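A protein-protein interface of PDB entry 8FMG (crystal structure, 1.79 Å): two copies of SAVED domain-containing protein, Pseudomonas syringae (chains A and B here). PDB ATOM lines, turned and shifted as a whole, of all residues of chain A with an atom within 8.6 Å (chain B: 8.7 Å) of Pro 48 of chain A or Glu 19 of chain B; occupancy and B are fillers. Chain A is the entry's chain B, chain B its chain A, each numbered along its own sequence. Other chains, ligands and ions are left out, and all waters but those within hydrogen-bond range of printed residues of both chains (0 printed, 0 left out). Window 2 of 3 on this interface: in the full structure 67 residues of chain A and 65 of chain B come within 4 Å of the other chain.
Arg 22 of chain B touches its own counterpart, Arg 22 of chain A. Positions printed for both chains: 22 and 54. Of the 15 pairs that touch across the chains among the printed residues, 1 has its exchanged pair printed and touching as well.
NH2 of Arg 22 of chain A touches CD1 of Trp 25 of chain B (3.5 Å). Ile 23 of chain B touches Thr 40 of chain A. Tyr 43 of chain A touches Glu 19 of chain B. CG1 of Ile 23 of chain B touches CG of Tyr 43 of chain A, at 3.6 Å. OH of Tyr 43 of chain A touches CG2 of Thr 80 of chain B, at 3.7 Å. NH2 of Arg 44 of chain A touches CG2 of Ile 23 of chain B (3.7 Å). Lys 47 of chain A touches Glu 19 of chain B (O to OE2, 3.7 Å). Pro 48 of chain A touches Glu 19 of chain B (CA to OE1, 3.4 Å). Trp 51 of chain A touches Arg 22 of chain B (CE2 to NE, 3.5 Å). Ile 23 of chain B touches Trp 51 of chain A (CD1 to CH2, 3.7 Å).
Of the 15 printed residues of chain A, 8 touch a printed residue of chain B. Printed residues of chain A that touch a printed residue of chain B: Arg 22, Thr 40, Tyr 43, Arg 44, Lys 47, Pro 48, Met 49 and Trp 51. Hydrophobic or aromatic side chains of chain A that line the printed part of chain B: Tyr 43, Pro 48 and Trp 51. Printed residues of chain B that touch a printed residue of chain A: Glu 19, Thr 20, Arg 22, Ile 23, Trp 25, Asn 78 and Thr 80. Among the printed residues, 15 pairs touch across the chains.
Printed residues of chain B within 4 Å of Met 49 of chain A: Glu 19. Of the printed residues of chain B, Lys 47 of chain A touches Glu 19. Of the printed residues of chain B, Thr 40 of chain A touches Ile 23 (3.99 Å). Printed residues of chain B within 4 Å of Arg 44 of chain A: Ile 23 and Thr 80. Printed residues of chain A within 4 Å of Thr 20 of chain B: Tyr 43 (2.9 Å). Leu 39 of chain A touches none of the printed residues of chain B. Ala 45 of chain A touches none of the printed residues of chain B. The nearest residue of chain A that does not touch Glu 19 of chain B is Trp 51 of chain A (4.9 Å). The nearest printed residue of chain A that does not touch Arg 22 of chain B is Met 49 of chain A (6.9 Å).
The backbone NH of Glu 19 of chain B lies within hydrogen-bond range of the side-chain amide oxygen of Asn 17 of chain B, 3.1 Å away. OD1 of Asn 17 of chain B is in hydrogen-bond range of N of Thr 20 of chain B (2.9 Å). OD1 of Asn 78 of chain B lies within hydrogen-bond range of ND2 of Asn 17 of chain B, at 2.5 Å. OG1 of Thr 20 of chain B sits at hydrogen-bond distance from OD1 of Asn 78 of chain B (2.9 Å). The backbone carbonyl oxygen (O) of Arg 22 of chain B is in hydrogen-bond range of the side-chain hydroxyl (OG1) of Thr 26 of chain B (2.8 Å). OG1 of Thr 40 of chain A sits at hydrogen-bond distance from NE of Arg 44 of chain A.
The backbone NH of Met 49 of chain A sits at hydrogen-bond distance from the side-chain carboxylate of Glu 19 of chain B. The side-chain hydroxyl (OG1) of Thr 20 of chain B lies within hydrogen-bond range of the side-chain hydroxyl (OH) of Tyr 43 of chain A (2.9 Å). The side-chain hydroxyl (OH) of Tyr 43 of chain A sits at hydrogen-bond distance from the backbone carbonyl oxygen (O) of Asn 78 of chain B (3.2 Å).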
ATOM      1  N   ARG A  22     -28.867  21.522 -23.795  1.00  0.00           N
ATOM      2  CA  ARG A  22     -29.992  20.718 -23.331  1.00  0.00           C
ATOM      3  C   ARG A  22     -31.215  20.892 -24.224  1.00  0.00           C
ATOM      4  O   ARG A  22     -31.991  19.945 -24.399  1.00  0.00           O
ATOM      5  CB  ARG A  22     -30.334  21.064 -21.882  1.00  0.00           C
ATOM      6  CG  ARG A  22     -31.435  20.186 -21.310  1.00  0.00           C
ATOM      7  CD  ARG A  22     -31.387  20.102 -19.791  1.00  0.00           C
ATOM      8  NE  ARG A  22     -32.409  19.198 -19.275  1.00  0.00           N
ATOM      9  CZ  ARG A  22     -32.580  18.907 -17.993  1.00  0.00           C
ATOM     10  NH1 ARG A  22     -31.813  19.439 -17.056  1.00  0.00           N
ATOM     11  NH2 ARG A  22     -33.543  18.059 -17.643  1.00  0.00           N
ATOM     12  N   LEU A  39     -26.813   8.701 -28.892  1.00  0.00           N
ATOM     13  CA  LEU A  39     -25.629   9.259 -28.253  1.00  0.00           C
ATOM     14  C   LEU A  39     -25.728   9.294 -26.730  1.00  0.00           C
ATOM     15  O   LEU A  39     -24.986  10.047 -26.086  1.00  0.00           O
ATOM     16  CB  LEU A  39     -25.360  10.668 -28.786  1.00  0.00           C
ATOM     17  CG  LEU A  39     -25.324  10.772 -30.311  1.00  0.00           C
ATOM     18  CD1 LEU A  39     -24.962  12.178 -30.741  1.00  0.00           C
ATOM     19  CD2 LEU A  39     -24.344   9.770 -30.891  1.00  0.00           C
ATOM     20  N   THR A  40     -26.614   8.493 -26.140  1.00  0.00           N
ATOM     21  CA  THR A  40     -26.670   8.329 -24.694  1.00  0.00           C
ATOM     22  C   THR A  40     -26.014   7.026 -24.237  1.00  0.00           C
ATOM     23  O   THR A  40     -26.328   6.532 -23.149  1.00  0.00           O
ATOM     24  CB  THR A  40     -28.118   8.381 -24.199  1.00  0.00           C
ATOM     25  OG1 THR A  40     -28.832   7.230 -24.671  1.00  0.00           O
ATOM     26  CG2 THR A  40     -28.812   9.647 -24.688  1.00  0.00           C
ATOM     27  N   PHE A  41     -25.097   6.472 -25.040  1.00  0.00           N
ATOM     28  CA  PHE A  41     -24.545   5.152 -24.744  1.00  0.00           C
ATOM     29  C   PHE A  41     -23.822   5.128 -23.400  1.00  0.00           C
ATOM     30  O   PHE A  41     -23.874   4.123 -22.681  1.00  0.00           O
ATOM     31  CB  PHE A  41     -23.608   4.699 -25.877  1.00  0.00           C
ATOM     32  CG  PHE A  41     -22.573   5.726 -26.265  1.00  0.00           C
ATOM     33  CD1 PHE A  41     -21.357   5.792 -25.601  1.00  0.00           C
ATOM     34  CD2 PHE A  41     -22.820   6.630 -27.291  1.00  0.00           C
ATOM     35  CE1 PHE A  41     -20.408   6.745 -25.948  1.00  0.00           C
ATOM     36  CE2 PHE A  41     -21.875   7.583 -27.641  1.00  0.00           C
ATOM     37  CZ  PHE A  41     -20.669   7.639 -26.970  1.00  0.00           C
ATOM     38  N   ASP A  42     -23.149   6.219 -23.030  1.00  0.00           N
ATOM     39  CA  ASP A  42     -22.354   6.186 -21.806  1.00  0.00           C
ATOM     40  C   ASP A  42     -23.238   6.075 -20.568  1.00  0.00           C
ATOM     41  O   ASP A  42     -22.890   5.363 -19.615  1.00  0.00           O
ATOM     42  CB  ASP A  42     -21.455   7.416 -21.717  1.00  0.00           C
ATOM     43  CG  ASP A  42     -20.108   7.187 -22.368  1.00  0.00           C
ATOM     44  OD1 ASP A  42     -19.643   6.026 -22.379  1.00  0.00           O
ATOM     45  OD2 ASP A  42     -19.517   8.163 -22.873  1.00  0.00           O
ATOM     46  N   TYR A  43     -24.381   6.767 -20.557  1.00  0.00           N
ATOM     47  CA  TYR A  43     -25.314   6.608 -19.445  1.00  0.00           C
ATOM     48  C   TYR A  43     -25.839   5.177 -19.379  1.00  0.00           C
ATOM     49  O   TYR A  43     -26.024   4.626 -18.286  1.00  0.00           O
ATOM     50  CB  TYR A  43     -26.475   7.596 -19.572  1.00  0.00           C
ATOM     51  CG  TYR A  43     -27.505   7.433 -18.474  1.00  0.00           C
ATOM     52  CD1 TYR A  43     -28.535   6.509 -18.594  1.00  0.00           C
ATOM     53  CD2 TYR A  43     -27.442   8.191 -17.310  1.00  0.00           C
ATOM     54  CE1 TYR A  43     -29.471   6.342 -17.593  1.00  0.00           C
ATOM     55  CE2 TYR A  43     -28.381   8.033 -16.301  1.00  0.00           C
ATOM     56  CZ  TYR A  43     -29.394   7.105 -16.450  1.00  0.00           C
ATOM     57  OH  TYR A  43     -30.334   6.930 -15.462  1.00  0.00           O
ATOM     58  N   ARG A  44     -26.094   4.562 -20.539  1.00  0.00           N
ATOM     59  CA  ARG A  44     -26.525   3.169 -20.551  1.00  0.00           C
ATOM     60  C   ARG A  44     -25.443   2.255 -19.987  1.00  0.00           C
ATOM     61  O   ARG A  44     -25.746   1.168 -19.480  1.00  0.00           O
ATOM     62  CB  ARG A  44     -26.884   2.723 -21.970  1.00  0.00           C
ATOM     63  CG  ARG A  44     -27.771   3.680 -22.750  1.00  0.00           C
ATOM     64  CD  ARG A  44     -29.056   3.993 -22.014  1.00  0.00           C
ATOM     65  NE  ARG A  44     -29.810   5.048 -22.676  1.00  0.00           N
ATOM     66  CZ  ARG A  44     -30.975   5.513 -22.248  1.00  0.00           C
ATOM     67  NH1 ARG A  44     -31.555   5.028 -21.166  1.00  0.00           N
ATOM     68  NH2 ARG A  44     -31.574   6.490 -22.923  1.00  0.00           N
ATOM     69  N   ALA A  45     -24.182   2.672 -20.084  1.00  0.00           N
ATOM     70  CA  ALA A  45     -23.045   1.916 -19.578  1.00  0.00           C
ATOM     71  C   ALA A  45     -22.703   2.268 -18.134  1.00  0.00           C
ATOM     72  O   ALA A  45     -21.664   1.827 -17.631  1.00  0.00           O
ATOM     73  CB  ALA A  45     -21.822   2.151 -20.468  1.00  0.00           C
ATOM     74  N   GLY A  46     -23.541   3.054 -17.465  1.00  0.00           N
ATOM     75  CA  GLY A  46     -23.300   3.408 -16.088  1.00  0.00           C
ATOM     76  C   GLY A  46     -22.276   4.498 -15.862  1.00  0.00           C
ATOM     77  O   GLY A  46     -21.873   4.714 -14.713  1.00  0.00           O
ATOM     78  N   LYS A  47     -21.852   5.195 -16.906  1.00  0.00           N
ATOM     79  CA  LYS A  47     -20.852   6.246 -16.794  1.00  0.00           C
ATOM     80  C   LYS A  47     -21.479   7.628 -16.912  1.00  0.00           C
ATOM     81  O   LYS A  47     -22.632   7.770 -17.333  1.00  0.00           O
ATOM     82  CB  LYS A  47     -19.774   6.078 -17.876  1.00  0.00           C
ATOM     83  CG  LYS A  47     -18.662   5.109 -17.489  1.00  0.00           C
ATOM     84  CD  LYS A  47     -17.741   4.793 -18.660  1.00  0.00           C
ATOM     85  CE  LYS A  47     -18.398   3.830 -19.639  1.00  0.00           C
ATOM     86  NZ  LYS A  47     -17.526   3.529 -20.810  1.00  0.00           N
ATOM     87  N   PRO A  48     -20.750   8.673 -16.522  1.00  0.00           N
ATOM     88  CA  PRO A  48     -21.271  10.034 -16.692  1.00  0.00           C
ATOM     89  C   PRO A  48     -21.262  10.453 -18.153  1.00  0.00           C
ATOM     90  O   PRO A  48     -20.439   9.999 -18.951  1.00  0.00           O
ATOM     91  CB  PRO A  48     -20.309  10.898 -15.864  1.00  0.00           C
ATOM     92  CG  PRO A  48     -19.565   9.936 -14.981  1.00  0.00           C
ATOM     93  CD  PRO A  48     -19.489   8.656 -15.760  1.00  0.00           C
ATOM     94  N   MET A  49     -22.189  11.341 -18.494  1.00  0.00           N
ATOM     95  CA  MET A  49     -22.277  11.856 -19.850  1.00  0.00           C
ATOM     96  C   MET A  49     -21.255  12.967 -20.072  1.00  0.00           C
ATOM     97  O   MET A  49     -20.917  13.722 -19.157  1.00  0.00           O
ATOM     98  CB  MET A  49     -23.682  12.391 -20.132  1.00  0.00           C
ATOM     99  CG  MET A  49     -24.766  11.328 -20.202  1.00  0.00           C
ATOM    100  SD  MET A  49     -24.600  10.223 -21.622  1.00  0.00           S
ATOM    101  CE  MET A  49     -24.542  11.390 -22.979  1.00  0.00           C
ATOM    102  N   LYS A  50     -20.761  13.057 -21.305  1.00  0.00           N
ATOM    103  CA  LYS A  50     -19.910  14.162 -21.753  1.00  0.00           C
ATOM    104  C   LYS A  50     -20.620  14.785 -22.959  1.00  0.00           C
ATOM    105  O   LYS A  50     -20.221  14.582 -24.109  1.00  0.00           O
ATOM    106  CB  LYS A  50     -18.464  13.688 -22.093  1.00  0.00           C
ATOM    107  CG  LYS A  50     -17.701  13.115 -20.890  1.00  0.00           C
ATOM    108  CD  LYS A  50     -16.203  12.942 -21.159  1.00  0.00           C
ATOM    109  CE  LYS A  50     -15.423  14.243 -20.964  1.00  0.00           C
ATOM    110  NZ  LYS A  50     -15.524  14.791 -19.577  1.00  0.00           N
ATOM    111  N   TRP A  51     -21.681  15.552 -22.681  1.00  0.00           N
ATOM    112  CA  TRP A  51     -22.590  15.987 -23.738  1.00  0.00           C
ATOM    113  C   TRP A  51     -21.869  16.794 -24.811  1.00  0.00           C
ATOM    114  O   TRP A  51     -22.301  16.809 -25.970  1.00  0.00           O
ATOM    115  CB  TRP A  51     -23.739  16.815 -23.143  1.00  0.00           C
ATOM    116  CG  TRP A  51     -24.409  16.207 -21.928  1.00  0.00           C
ATOM    117  CD1 TRP A  51     -24.005  16.332 -20.629  1.00  0.00           C
ATOM    118  CD2 TRP A  51     -25.602  15.405 -21.899  1.00  0.00           C
ATOM    119  NE1 TRP A  51     -24.862  15.653 -19.796  1.00  0.00           N
ATOM    120  CE2 TRP A  51     -25.851  15.078 -20.549  1.00  0.00           C
ATOM    121  CE3 TRP A  51     -26.479  14.934 -22.879  1.00  0.00           C
ATOM    122  CZ2 TRP A  51     -26.937  14.298 -20.156  1.00  0.00           C
ATOM    123  CZ3 TRP A  51     -27.559  14.157 -22.485  1.00  0.00           C
ATOM    124  CH2 TRP A  51     -27.779  13.848 -21.138  1.00  0.00           C
ATOM    125  N   VAL A  54     -19.405  13.751 -26.792  1.00  0.00           N
ATOM    126  CA  VAL A  54     -20.042  12.717 -27.603  1.00  0.00           C
ATOM    127  C   VAL A  54     -20.849  13.294 -28.755  1.00  0.00           C
ATOM    128  O   VAL A  54     -21.305  12.538 -29.621  1.00  0.00           O
ATOM    129  CB  VAL A  54     -20.968  11.814 -26.764  1.00  0.00           C
ATOM    130  CG1 VAL A  54     -20.196  11.177 -25.612  1.00  0.00           C
ATOM    131  CG2 VAL A  54     -22.168  12.600 -26.251  1.00  0.00           C
ATOM    132  N   THR B  16     -34.250  10.761  -7.569  1.00  0.00           N
ATOM    133  CA  THR B  16     -33.663  10.651  -8.898  1.00  0.00           C
ATOM    134  C   THR B  16     -32.668  11.787  -9.113  1.00  0.00           C
ATOM    135  O   THR B  16     -32.982  12.956  -8.867  1.00  0.00           O
ATOM    136  CB  THR B  16     -34.757  10.697  -9.962  1.00  0.00           C
ATOM    137  OG1 THR B  16     -35.704   9.649  -9.720  1.00  0.00           O
ATOM    138  CG2 THR B  16     -34.171  10.536 -11.361  1.00  0.00           C
ATOM    139  N   ASN B  17     -31.470  11.446  -9.575  1.00  0.00           N
ATOM    140  CA  ASN B  17     -30.440  12.457  -9.748  1.00  0.00           C
ATOM    141  C   ASN B  17     -30.659  13.223 -11.053  1.00  0.00           C
ATOM    142  O   ASN B  17     -31.484  12.855 -11.897  1.00  0.00           O
ATOM    143  CB  ASN B  17     -29.051  11.824  -9.721  1.00  0.00           C
ATOM    144  CG  ASN B  17     -28.847  10.815 -10.830  1.00  0.00           C
ATOM    145  OD1 ASN B  17     -28.814  11.170 -12.006  1.00  0.00           O
ATOM    146  ND2 ASN B  17     -28.696   9.549 -10.457  1.00  0.00           N
ATOM    147  N   ASP B  18     -29.893  14.306 -11.215  1.00  0.00           N
ATOM    148  CA  ASP B  18     -30.118  15.212 -12.334  1.00  0.00           C
ATOM    149  C   ASP B  18     -29.706  14.601 -13.665  1.00  0.00           C
ATOM    150  O   ASP B  18     -30.297  14.927 -14.701  1.00  0.00           O
ATOM    151  CB  ASP B  18     -29.356  16.519 -12.123  1.00  0.00           C
ATOM    152  CG  ASP B  18     -30.014  17.407 -11.101  1.00  0.00           C
ATOM    153  OD1 ASP B  18     -31.054  16.985 -10.558  1.00  0.00           O
ATOM    154  OD2 ASP B  18     -29.501  18.514 -10.845  1.00  0.00           O
ATOM    155  N   GLU B  19     -28.683  13.747 -13.669  1.00  0.00           N
ATOM    156  CA  GLU B  19     -28.268  13.127 -14.922  1.00  0.00           C
ATOM    157  C   GLU B  19     -29.377  12.244 -15.475  1.00  0.00           C
ATOM    158  O   GLU B  19     -29.716  12.314 -16.662  1.00  0.00           O
ATOM    159  CB  GLU B  19     -26.990  12.321 -14.710  1.00  0.00           C
ATOM    160  CG  GLU B  19     -26.606  11.486 -15.915  1.00  0.00           C
ATOM    161  CD  GLU B  19     -25.224  10.886 -15.793  1.00  0.00           C
ATOM    162  OE1 GLU B  19     -24.240  11.608 -16.057  1.00  0.00           O
ATOM    163  OE2 GLU B  19     -25.123   9.694 -15.430  1.00  0.00           O
ATOM    164  N   THR B  20     -29.963  11.410 -14.616  1.00  0.00           N
ATOM    165  CA  THR B  20     -31.073  10.557 -15.028  1.00  0.00           C
ATOM    166  C   THR B  20     -32.237  11.383 -15.555  1.00  0.00           C
ATOM    167  O   THR B  20     -32.817  11.064 -16.599  1.00  0.00           O
ATOM    168  CB  THR B  20     -31.512   9.691 -13.845  1.00  0.00           C
ATOM    169  OG1 THR B  20     -30.381   8.959 -13.355  1.00  0.00           O
ATOM    170  CG2 THR B  20     -32.611   8.726 -14.250  1.00  0.00           C
ATOM    171  N   LYS B  21     -32.604  12.446 -14.838  1.00  0.00           N
ATOM    172  CA  LYS B  21     -33.680  13.305 -15.318  1.00  0.00           C
ATOM    173  C   LYS B  21     -33.355  13.867 -16.696  1.00  0.00           C
ATOM    174  O   LYS B  21     -34.220  13.907 -17.579  1.00  0.00           O
ATOM    175  CB  LYS B  21     -33.941  14.435 -14.324  1.00  0.00           C
ATOM    176  CG  LYS B  21     -34.537  13.949 -13.018  1.00  0.00           C
ATOM    177  CD  LYS B  21     -34.976  15.099 -12.131  1.00  0.00           C
ATOM    178  CE  LYS B  21     -35.540  14.575 -10.819  1.00  0.00           C
ATOM    179  NZ  LYS B  21     -35.920  15.665  -9.882  1.00  0.00           N
ATOM    180  N   ARG B  22     -32.109  14.294 -16.908  1.00  0.00           N
ATOM    181  CA  ARG B  22     -31.738  14.818 -18.217  1.00  0.00           C
ATOM    182  C   ARG B  22     -31.848  13.748 -19.294  1.00  0.00           C
ATOM    183  O   ARG B  22     -32.184  14.056 -20.442  1.00  0.00           O
ATOM    184  CB  ARG B  22     -30.326  15.398 -18.154  1.00  0.00           C
ATOM    185  CG  ARG B  22     -29.961  16.275 -19.334  1.00  0.00           C
ATOM    186  CD  ARG B  22     -28.763  17.152 -19.008  1.00  0.00           C
ATOM    187  NE  ARG B  22     -28.138  17.702 -20.204  1.00  0.00           N
ATOM    188  CZ  ARG B  22     -27.069  18.484 -20.199  1.00  0.00           C
ATOM    189  NH1 ARG B  22     -26.477  18.837 -19.073  1.00  0.00           N
ATOM    190  NH2 ARG B  22     -26.581  18.926 -21.354  1.00  0.00           N
ATOM    191  N   ILE B  23     -31.589  12.487 -18.942  1.00  0.00           N
ATOM    192  CA  ILE B  23     -31.781  11.395 -19.893  1.00  0.00           C
ATOM    193  C   ILE B  23     -33.266  11.208 -20.185  1.00  0.00           C
ATOM    194  O   ILE B  23     -33.681  11.118 -21.347  1.00  0.00           O
ATOM    195  CB  ILE B  23     -31.140  10.103 -19.352  1.00  0.00           C
ATOM    196  CG1 ILE B  23     -29.610  10.224 -19.371  1.00  0.00           C
ATOM    197  CG2 ILE B  23     -31.597   8.886 -20.144  1.00  0.00           C
ATOM    198  CD1 ILE B  23     -29.004  10.350 -20.762  1.00  0.00           C
ATOM    199  N   VAL B  24     -34.086  11.139 -19.135  1.00  0.00           N
ATOM    200  CA  VAL B  24     -35.533  11.034 -19.318  1.00  0.00           C
ATOM    201  C   VAL B  24     -36.025  12.113 -20.273  1.00  0.00           C
ATOM    202  O   VAL B  24     -36.797  11.843 -21.200  1.00  0.00           O
ATOM    203  CB  VAL B  24     -36.245  11.106 -17.956  1.00  0.00           C
ATOM    204  CG1 VAL B  24     -37.709  11.473 -18.115  1.00  0.00           C
ATOM    205  CG2 VAL B  24     -36.097   9.776 -17.227  1.00  0.00           C
ATOM    206  N   TRP B  25     -35.585  13.353 -20.061  1.00  0.00           N
ATOM    207  CA  TRP B  25     -35.994  14.432 -20.955  1.00  0.00           C
ATOM    208  C   TRP B  25     -35.521  14.178 -22.381  1.00  0.00           C
ATOM    209  O   TRP B  25     -36.230  14.501 -23.344  1.00  0.00           O
ATOM    210  CB  TRP B  25     -35.468  15.775 -20.441  1.00  0.00           C
ATOM    211  CG  TRP B  25     -36.384  16.409 -19.447  1.00  0.00           C
ATOM    212  CD1 TRP B  25     -36.414  16.182 -18.104  1.00  0.00           C
ATOM    213  CD2 TRP B  25     -37.413  17.368 -19.716  1.00  0.00           C
ATOM    214  NE1 TRP B  25     -37.398  16.941 -17.517  1.00  0.00           N
ATOM    215  CE2 TRP B  25     -38.025  17.677 -18.486  1.00  0.00           C
ATOM    216  CE3 TRP B  25     -37.877  17.997 -20.876  1.00  0.00           C
ATOM    217  CZ2 TRP B  25     -39.077  18.588 -18.382  1.00  0.00           C
ATOM    218  CZ3 TRP B  25     -38.921  18.901 -20.771  1.00  0.00           C
ATOM    219  CH2 TRP B  25     -39.507  19.187 -19.531  1.00  0.00           C
ATOM    220  N   THR B  26     -34.330  13.590 -22.538  1.00  0.00           N
ATOM    221  CA  THR B  26     -33.796  13.340 -23.874  1.00  0.00           C
ATOM    222  C   THR B  26     -34.507  12.163 -24.539  1.00  0.00           C
ATOM    223  O   THR B  26     -34.892  12.239 -25.714  1.00  0.00           O
ATOM    224  CB  THR B  26     -32.290  13.073 -23.796  1.00  0.00           C
ATOM    225  OG1 THR B  26     -31.629  14.181 -23.178  1.00  0.00           O
ATOM    226  CG2 THR B  26     -31.702  12.856 -25.189  1.00  0.00           C
ATOM    227  N   VAL B  54     -40.530  14.247 -13.907  1.00  0.00           N
ATOM    228  CA  VAL B  54     -40.051  12.872 -14.021  1.00  0.00           C
ATOM    229  C   VAL B  54     -40.822  12.042 -12.998  1.00  0.00           C
ATOM    230  O   VAL B  54     -40.589  12.153 -11.793  1.00  0.00           O
ATOM    231  CB  VAL B  54     -38.536  12.781 -13.796  1.00  0.00           C
ATOM    232  CG1 VAL B  54     -38.063  11.333 -13.846  1.00  0.00           C
ATOM    233  CG2 VAL B  54     -37.799  13.630 -14.829  1.00  0.00           C
ATOM    234  N   ASN B  78     -33.261   5.407 -10.167  1.00  0.00           N
ATOM    235  CA  ASN B  78     -32.621   5.914 -11.376  1.00  0.00           C
ATOM    236  C   ASN B  78     -32.724   4.919 -12.528  1.00  0.00           C
ATOM    237  O   ASN B  78     -31.909   4.951 -13.454  1.00  0.00           O
ATOM    238  CB  ASN B  78     -31.159   6.272 -11.092  1.00  0.00           C
ATOM    239  CG  ASN B  78     -31.026   7.437 -10.128  1.00  0.00           C
ATOM    240  OD1 ASN B  78     -31.024   8.598 -10.537  1.00  0.00           O
ATOM    241  ND2 ASN B  78     -30.926   7.131  -8.839  1.00  0.00           N
ATOM    242  N   THR B  80     -34.433   4.120 -15.745  1.00  0.00           N
ATOM    243  CA  THR B  80     -35.232   4.891 -16.696  1.00  0.00           C
ATOM    244  C   THR B  80     -36.431   4.114 -17.222  1.00  0.00           C
ATOM    245  O   THR B  80     -37.383   4.729 -17.716  1.00  0.00           O
ATOM    246  CB  THR B  80     -34.389   5.349 -17.888  1.00  0.00           C
ATOM    247  OG1 THR B  80     -33.682   4.224 -18.437  1.00  0.00           O
ATOM    248  CG2 THR B  80     -33.401   6.414 -17.469  1.00  0.00           C
ATOM    249  N   LEU B  83     -39.196   5.399 -15.076  1.00  0.00           N
ATOM    250  CA  LEU B  83     -39.404   6.838 -15.053  1.00  0.00           C
ATOM    251  C   LEU B  83     -40.023   7.284 -16.368  1.00  0.00           C
ATOM    252  O   LEU B  83     -39.540   6.918 -17.445  1.00  0.00           O
ATOM    253  CB  LEU B  83     -38.082   7.576 -14.818  1.00  0.00           C
ATOM    254  CG  LEU B  83     -37.295   7.161 -13.576  1.00  0.00           C
ATOM    255  CD1 LEU B  83     -35.849   7.623 -13.692  1.00  0.00           C
ATOM    256  CD2 LEU B  83     -37.933   7.717 -12.313  1.00  0.00           C
